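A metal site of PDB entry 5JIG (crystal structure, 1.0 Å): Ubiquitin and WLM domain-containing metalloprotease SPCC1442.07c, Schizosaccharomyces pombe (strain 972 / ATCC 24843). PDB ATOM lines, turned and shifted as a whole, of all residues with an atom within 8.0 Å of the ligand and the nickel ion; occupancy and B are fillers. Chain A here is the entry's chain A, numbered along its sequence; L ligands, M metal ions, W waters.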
ATOM      1  N   MET A  50      10.951   4.337  16.916  1.00  0.00           N
ATOM      2  CA  MET A  50      12.310   4.367  17.277  1.00  0.00           C
ATOM      3  C   MET A  50      13.145   4.560  15.991  1.00  0.00           C
ATOM      4  O   MET A  50      12.874   3.970  14.941  1.00  0.00           O
ATOM      5  CB  MET A  50      12.701   3.062  17.930  1.00  0.00           C
ATOM      6  CG  MET A  50      13.994   2.943  18.644  1.00  0.00           C
ATOM      7  SD  MET A  50      14.061   1.321  19.484  1.00  0.00           S
ATOM      8  CE  MET A  50      15.789   1.355  19.985  1.00  0.00           C
ATOM      9  N   THR A  62      17.973  -3.930  20.378  1.00  0.00           N
ATOM     10  CA  THR A  62      17.540  -2.564  20.338  1.00  0.00           C
ATOM     11  C   THR A  62      16.309  -2.369  19.461  1.00  0.00           C
ATOM     12  O   THR A  62      16.287  -1.562  18.577  1.00  0.00           O
ATOM     13  CB  THR A  62      18.684  -1.736  19.810  1.00  0.00           C
ATOM     14  OG1 THR A  62      19.121  -2.411  18.640  1.00  0.00           O
ATOM     15  CG2 THR A  62      19.806  -1.679  20.860  1.00  0.00           C
ATOM     16  N   LEU A  63      15.244  -3.099  19.726  1.00  0.00           N
ATOM     17  CA  LEU A  63      14.045  -2.977  18.936  1.00  0.00           C
ATOM     18  C   LEU A  63      12.908  -2.242  19.601  1.00  0.00           C
ATOM     19  O   LEU A  63      11.908  -1.934  18.936  1.00  0.00           O
ATOM     20  CB  LEU A  63      13.583  -4.289  18.384  1.00  0.00           C
ATOM     21  CG  LEU A  63      14.642  -4.914  17.451  1.00  0.00           C
ATOM     22  CD1 LEU A  63      14.190  -6.257  17.066  1.00  0.00           C
ATOM     23  CD2 LEU A  63      14.939  -4.112  16.195  1.00  0.00           C
ATOM     24  N   GLY A  64      13.053  -1.938  20.869  1.00  0.00           N
ATOM     25  CA  GLY A  64      12.063  -1.172  21.588  1.00  0.00           C
ATOM     26  C   GLY A  64      12.695  -0.549  22.813  1.00  0.00           C
ATOM     27  O   GLY A  64      13.801  -0.913  23.191  1.00  0.00           O
ATOM     28  N   LEU A  65      11.962   0.387  23.403  1.00  0.00           N
ATOM     29  CA  LEU A  65      12.370   1.105  24.608  1.00  0.00           C
ATOM     30  C   LEU A  65      11.153   1.379  25.466  1.00  0.00           C
ATOM     31  O   LEU A  65      10.081   1.641  24.949  1.00  0.00           O
ATOM     32  CB  LEU A  65      12.971   2.490  24.249  1.00  0.00           C
ATOM     33  CG  LEU A  65      14.190   2.470  23.437  1.00  0.00           C
ATOM     34  CD1 LEU A  65      14.493   3.856  22.806  1.00  0.00           C
ATOM     35  CD2 LEU A  65      15.361   1.990  24.265  1.00  0.00           C
ATOM     36  N   ASN A  66      11.346   1.363  26.786  1.00  0.00           N
ATOM     37  CA  ASN A  66      10.351   1.837  27.714  1.00  0.00           C
ATOM     38  C   ASN A  66      11.018   2.851  28.634  1.00  0.00           C
ATOM     39  O   ASN A  66      11.886   2.493  29.431  1.00  0.00           O
ATOM     40  CB  ASN A  66       9.774   0.715  28.534  1.00  0.00           C
ATOM     41  CG  ASN A  66       8.711   1.192  29.504  1.00  0.00           C
ATOM     42  OD1 ASN A  66       8.872   2.276  30.069  1.00  0.00           O
ATOM     43  ND2 ASN A  66       7.620   0.465  29.665  1.00  0.00           N
ATOM     44  N   HIS A  67      10.656   4.119  28.474  1.00  0.00           N
ATOM     45  CA  HIS A  67      11.205   5.187  29.297  1.00  0.00           C
ATOM     46  C   HIS A  67      10.292   5.459  30.500  1.00  0.00           C
ATOM     47  O   HIS A  67       9.112   5.742  30.348  1.00  0.00           O
ATOM     48  CB  HIS A  67      11.388   6.460  28.502  1.00  0.00           C
ATOM     49  CG  HIS A  67      12.162   6.296  27.252  1.00  0.00           C
ATOM     50  ND1 HIS A  67      13.450   5.826  27.236  1.00  0.00           N
ATOM     51  CD2 HIS A  67      11.819   6.572  25.985  1.00  0.00           C
ATOM     52  CE1 HIS A  67      13.858   5.840  25.977  1.00  0.00           C
ATOM     53  NE2 HIS A  67      12.889   6.287  25.200  1.00  0.00           N
ATOM     54  N   GLU A  74       8.943   3.310  22.785  1.00  0.00           N
ATOM     55  CA  GLU A  74       9.405   3.445  21.404  1.00  0.00           C
ATOM     56  C   GLU A  74       9.535   2.045  20.787  1.00  0.00           C
ATOM     57  O   GLU A  74       9.880   1.074  21.478  1.00  0.00           O
ATOM     58  CB  GLU A  74      10.717   4.149  21.248  1.00  0.00           C
ATOM     59  CG  GLU A  74      10.862   5.409  22.052  1.00  0.00           C
ATOM     60  CD  GLU A  74      12.038   6.247  21.648  1.00  0.00           C
ATOM     61  OE1 GLU A  74      12.398   6.232  20.450  1.00  0.00           O
ATOM     62  OE2 GLU A  74      12.581   6.927  22.552  1.00  0.00           O
ATOM     63  N   THR A  94       7.435  -7.274  20.609  1.00  0.00           N
ATOM     64  CA  THR A  94       8.297  -6.264  21.199  1.00  0.00           C
ATOM     65  C   THR A  94       7.492  -5.246  22.021  1.00  0.00           C
ATOM     66  O   THR A  94       7.892  -4.886  23.118  1.00  0.00           O
ATOM     67  CB  THR A  94       9.156  -5.575  20.151  1.00  0.00           C
ATOM     68  OG1 THR A  94      10.012  -6.554  19.559  1.00  0.00           O
ATOM     69  CG2 THR A  94       9.956  -4.419  20.710  1.00  0.00           C
ATOM     70  N   HIS A  97       6.725  -6.820  25.285  1.00  0.00           N
ATOM     71  CA  HIS A  97       7.922  -6.756  26.076  1.00  0.00           C
ATOM     72  C   HIS A  97       8.042  -5.374  26.736  1.00  0.00           C
ATOM     73  O   HIS A  97       8.256  -5.272  27.965  1.00  0.00           O
ATOM     74  CB  HIS A  97       9.137  -7.066  25.178  1.00  0.00           C
ATOM     75  CG  HIS A  97      10.443  -6.926  25.850  1.00  0.00           C
ATOM     76  ND1 HIS A  97      11.324  -7.980  25.981  1.00  0.00           N
ATOM     77  CD2 HIS A  97      11.081  -5.874  26.421  1.00  0.00           C
ATOM     78  CE1 HIS A  97      12.411  -7.536  26.589  1.00  0.00           C
ATOM     79  NE2 HIS A  97      12.303  -6.265  26.885  1.00  0.00           N
ATOM     80  N   GLU A  98       7.920  -4.314  25.947  1.00  0.00           N
ATOM     81  CA  GLU A  98       8.041  -2.983  26.525  1.00  0.00           C
ATOM     82  C   GLU A  98       6.950  -2.714  27.565  1.00  0.00           C
ATOM     83  O   GLU A  98       7.247  -2.111  28.610  1.00  0.00           O
ATOM     84  CB  GLU A  98       8.082  -1.884  25.482  1.00  0.00           C
ATOM     85  CG  GLU A  98       9.118  -2.053  24.368  1.00  0.00           C
ATOM     86  CD  GLU A  98      10.449  -2.436  24.742  1.00  0.00           C
ATOM     87  OE1 GLU A  98      10.850  -2.220  25.892  1.00  0.00           O
ATOM     88  OE2 GLU A  98      11.136  -2.955  23.812  1.00  0.00           O
ATOM     89  N   LEU A  99       5.736  -3.116  27.323  1.00  0.00           N
ATOM     90  CA  LEU A  99       4.687  -2.940  28.327  1.00  0.00           C
ATOM     91  C   LEU A  99       5.010  -3.662  29.631  1.00  0.00           C
ATOM     92  O   LEU A  99       4.685  -3.165  30.709  1.00  0.00           O
ATOM     93  CB  LEU A  99       3.349  -3.401  27.779  1.00  0.00           C
ATOM     94  CG  LEU A  99       2.722  -2.482  26.716  1.00  0.00           C
ATOM     95  CD1 LEU A  99       1.569  -3.178  26.058  1.00  0.00           C
ATOM     96  CD2 LEU A  99       2.249  -1.158  27.325  1.00  0.00           C
ATOM     97  N   THR A 100       5.641  -4.845  29.534  1.00  0.00           N
ATOM     98  CA  THR A 100       6.014  -5.589  30.719  1.00  0.00           C
ATOM     99  C   THR A 100       6.942  -4.778  31.602  1.00  0.00           C
ATOM    100  O   THR A 100       6.929  -4.865  32.835  1.00  0.00           O
ATOM    101  CB  THR A 100       6.654  -6.939  30.289  1.00  0.00           C
ATOM    102  OG1 THR A 100       5.766  -7.675  29.481  1.00  0.00           O
ATOM    103  CG2 THR A 100       6.926  -7.812  31.489  1.00  0.00           C
ATOM    104  N   HIS A 101       7.802  -3.949  30.997  1.00  0.00           N
ATOM    105  CA  HIS A 101       8.681  -3.045  31.700  1.00  0.00           C
ATOM    106  C   HIS A 101       7.938  -1.911  32.436  1.00  0.00           C
ATOM    107  O   HIS A 101       8.568  -1.183  33.210  1.00  0.00           O
ATOM    108  CB  HIS A 101       9.719  -2.425  30.782  1.00  0.00           C
ATOM    109  CG  HIS A 101      10.842  -3.351  30.367  1.00  0.00           C
ATOM    110  ND1 HIS A 101      11.664  -3.981  31.256  1.00  0.00           N
ATOM    111  CD2 HIS A 101      11.348  -3.602  29.136  1.00  0.00           C
ATOM    112  CE1 HIS A 101      12.599  -4.620  30.570  1.00  0.00           C
ATOM    113  NE2 HIS A 101      12.467  -4.401  29.287  1.00  0.00           N
ATOM    114  N   HIS A 104       8.248  -4.469  35.559  1.00  0.00           N
ATOM    115  CA  HIS A 104       9.512  -5.136  35.904  1.00  0.00           C
ATOM    116  C   HIS A 104      10.667  -4.479  35.124  1.00  0.00           C
ATOM    117  O   HIS A 104      10.631  -4.497  33.858  1.00  0.00           O
ATOM    118  CB  HIS A 104       9.410  -6.617  35.562  1.00  0.00           C
ATOM    119  CG  HIS A 104       8.342  -7.320  36.347  1.00  0.00           C
ATOM    120  ND1 HIS A 104       8.425  -7.476  37.732  1.00  0.00           N
ATOM    121  CD2 HIS A 104       7.140  -7.833  35.964  1.00  0.00           C
ATOM    122  CE1 HIS A 104       7.315  -8.057  38.128  1.00  0.00           C
ATOM    123  NE2 HIS A 104       6.524  -8.303  37.089  1.00  0.00           N
ATOM    124  N   GLY A 105      11.676  -3.986  35.792  1.00  0.00           N
ATOM    125  CA  GLY A 105      12.773  -3.333  35.139  1.00  0.00           C
ATOM    126  C   GLY A 105      13.775  -4.223  34.451  1.00  0.00           C
ATOM    127  O   GLY A 105      14.230  -3.904  33.317  1.00  0.00           O
ATOM    128  N   GLU A 106      14.037  -5.339  35.098  1.00  0.00           N
ATOM    129  CA  GLU A 106      14.993  -6.324  34.642  1.00  0.00           C
ATOM    130  C   GLU A 106      14.238  -7.498  33.953  1.00  0.00           C
ATOM    131  O   GLU A 106      13.125  -7.793  34.276  1.00  0.00           O
ATOM    132  CB  GLU A 106      15.787  -6.925  35.829  1.00  0.00           C
ATOM    133  CG  GLU A 106      16.692  -5.889  36.461  1.00  0.00           C
ATOM    134  CD  GLU A 106      17.628  -5.194  35.473  1.00  0.00           C
ATOM    135  OE1 GLU A 106      18.328  -5.886  34.754  1.00  0.00           O
ATOM    136  OE2 GLU A 106      17.618  -3.939  35.343  1.00  0.00           O
ATOM    137  N   HIS A 107      14.985  -8.163  33.030  1.00  0.00           N
ATOM    138  CA  HIS A 107      14.458  -9.324  32.340  1.00  0.00           C
ATOM    139  C   HIS A 107      14.606 -10.592  33.176  1.00  0.00           C
ATOM    140  O   HIS A 107      15.209 -11.569  32.746  1.00  0.00           O
ATOM    141  CB  HIS A 107      15.072  -9.499  30.967  1.00  0.00           C
ATOM    142  CG  HIS A 107      15.034  -8.290  30.070  1.00  0.00           C
ATOM    143  ND1 HIS A 107      16.194  -7.736  29.613  1.00  0.00           N
ATOM    144  CD2 HIS A 107      14.065  -7.515  29.585  1.00  0.00           C
ATOM    145  CE1 HIS A 107      15.927  -6.711  28.851  1.00  0.00           C
ATOM    146  NE2 HIS A 107      14.645  -6.537  28.841  1.00  0.00           N
ATOM    147  N   PHE A 111       9.557 -10.813  35.227  1.00  0.00           N
ATOM    148  CA  PHE A 111       9.348 -10.197  33.890  1.00  0.00           C
ATOM    149  C   PHE A 111       8.830 -11.189  32.926  1.00  0.00           C
ATOM    150  O   PHE A 111       7.818 -10.988  32.278  1.00  0.00           O
ATOM    151  CB  PHE A 111      10.672  -9.565  33.433  1.00  0.00           C
ATOM    152  CG  PHE A 111      10.587  -8.937  32.026  1.00  0.00           C
ATOM    153  CD1 PHE A 111      10.399  -7.580  31.840  1.00  0.00           C
ATOM    154  CD2 PHE A 111      10.689  -9.739  30.865  1.00  0.00           C
ATOM    155  CE1 PHE A 111      10.220  -7.054  30.558  1.00  0.00           C
ATOM    156  CE2 PHE A 111      10.512  -9.222  29.603  1.00  0.00           C
ATOM    157  CZ  PHE A 111      10.273  -7.883  29.458  1.00  0.00           C
ATOM    158  N   TRP A 112       9.547 -12.359  32.778  1.00  0.00           N
ATOM    159  CA  TRP A 112       9.146 -13.272  31.736  1.00  0.00           C
ATOM    160  C   TRP A 112       7.829 -13.983  32.052  1.00  0.00           C
ATOM    161  O   TRP A 112       7.068 -14.305  31.134  1.00  0.00           O
ATOM    162  CB  TRP A 112      10.272 -14.239  31.410  1.00  0.00           C
ATOM    163  CG  TRP A 112      11.425 -13.581  30.725  1.00  0.00           C
ATOM    164  CD1 TRP A 112      12.681 -13.406  31.225  1.00  0.00           C
ATOM    165  CD2 TRP A 112      11.413 -12.964  29.438  1.00  0.00           C
ATOM    166  NE1 TRP A 112      13.450 -12.715  30.339  1.00  0.00           N
ATOM    167  CE2 TRP A 112      12.714 -12.445  29.228  1.00  0.00           C
ATOM    168  CE3 TRP A 112      10.465 -12.822  28.413  1.00  0.00           C
ATOM    169  CZ2 TRP A 112      13.045 -11.797  28.048  1.00  0.00           C
ATOM    170  CZ3 TRP A 112      10.820 -12.165  27.259  1.00  0.00           C
ATOM    171  CH2 TRP A 112      12.071 -11.664  27.089  1.00  0.00           C
HETATM  172  O1  LIG L   1      13.164  -3.301  26.509  1.00  0.00           O
HETATM  173  O2  LIG L   1      14.071  -2.551  26.124  1.00  0.00           O
HETATM  174 NI    NI M   1      13.703  -4.997  27.735  1.00  0.00          NI
HETATM  175  O   HOH W   1      13.015  -4.818  23.656  1.00  0.00           O
HETATM  176  O   HOH W   2      15.200  -3.574  28.271  1.00  0.00           O
HETATM  177  O   HOH W   3      14.971  -5.296  25.989  1.00  0.00           O
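An oxygen (O1) of the ligand sits close to the side-chain carboxylate (OE1) of Glu 98, 2.6 Å away.
ND1 of His 101 sits close to O of Gly 105 (3.3 Å).
A ring nitrogen (ND1) of His 101 lies within hydrogen-bond range of the backbone carbonyl oxygen (O) of His 104 (2.8 Å).
The indole nitrogen of Trp 112 lies within hydrogen-bond range of the backbone carbonyl oxygen of His 107 (3.2 Å).
The side-chain carboxylate of Glu 98 is in hydrogen-bond range of the backbone NH of Leu 65 (3.5 Å).
The backbone carbonyl oxygen (O) of Glu 98 lies within hydrogen-bond range of the side-chain amide nitrogen (ND2) of Asn 66, 2.8 Å away.
The backbone NH of Gly 64 lies within hydrogen-bond range of the side-chain sulfur of Met 50, 3.7 Å away.
O of Gly 64 sits close to O2 of the ligand (3.4 Å).
Four residues have an atom within 4 Å of the ligand: Gly 64, His 97, Glu 98 and His 101.
The nearest printed residue that does not touch the ligand is His 107 (4.3 Å).
Within 4 Å of the nickel ion: His 97, His 101 and His 107.
The nickel ion is bound by NE2 of His 101 (2.1 Å).
The nickel ion is bound by NE2 of His 97.
The nickel ion is bound by a ring nitrogen (NE2) of His 107 (2.1 Å).
The nickel ion is bound by water W2 (2.1 Å).
O1 of the ligand is bound to the nickel ion (2.2 Å).
The nickel ion is bound by water W3, at 2.2 Å.
The nickel ion has six donor atoms within binding distance.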
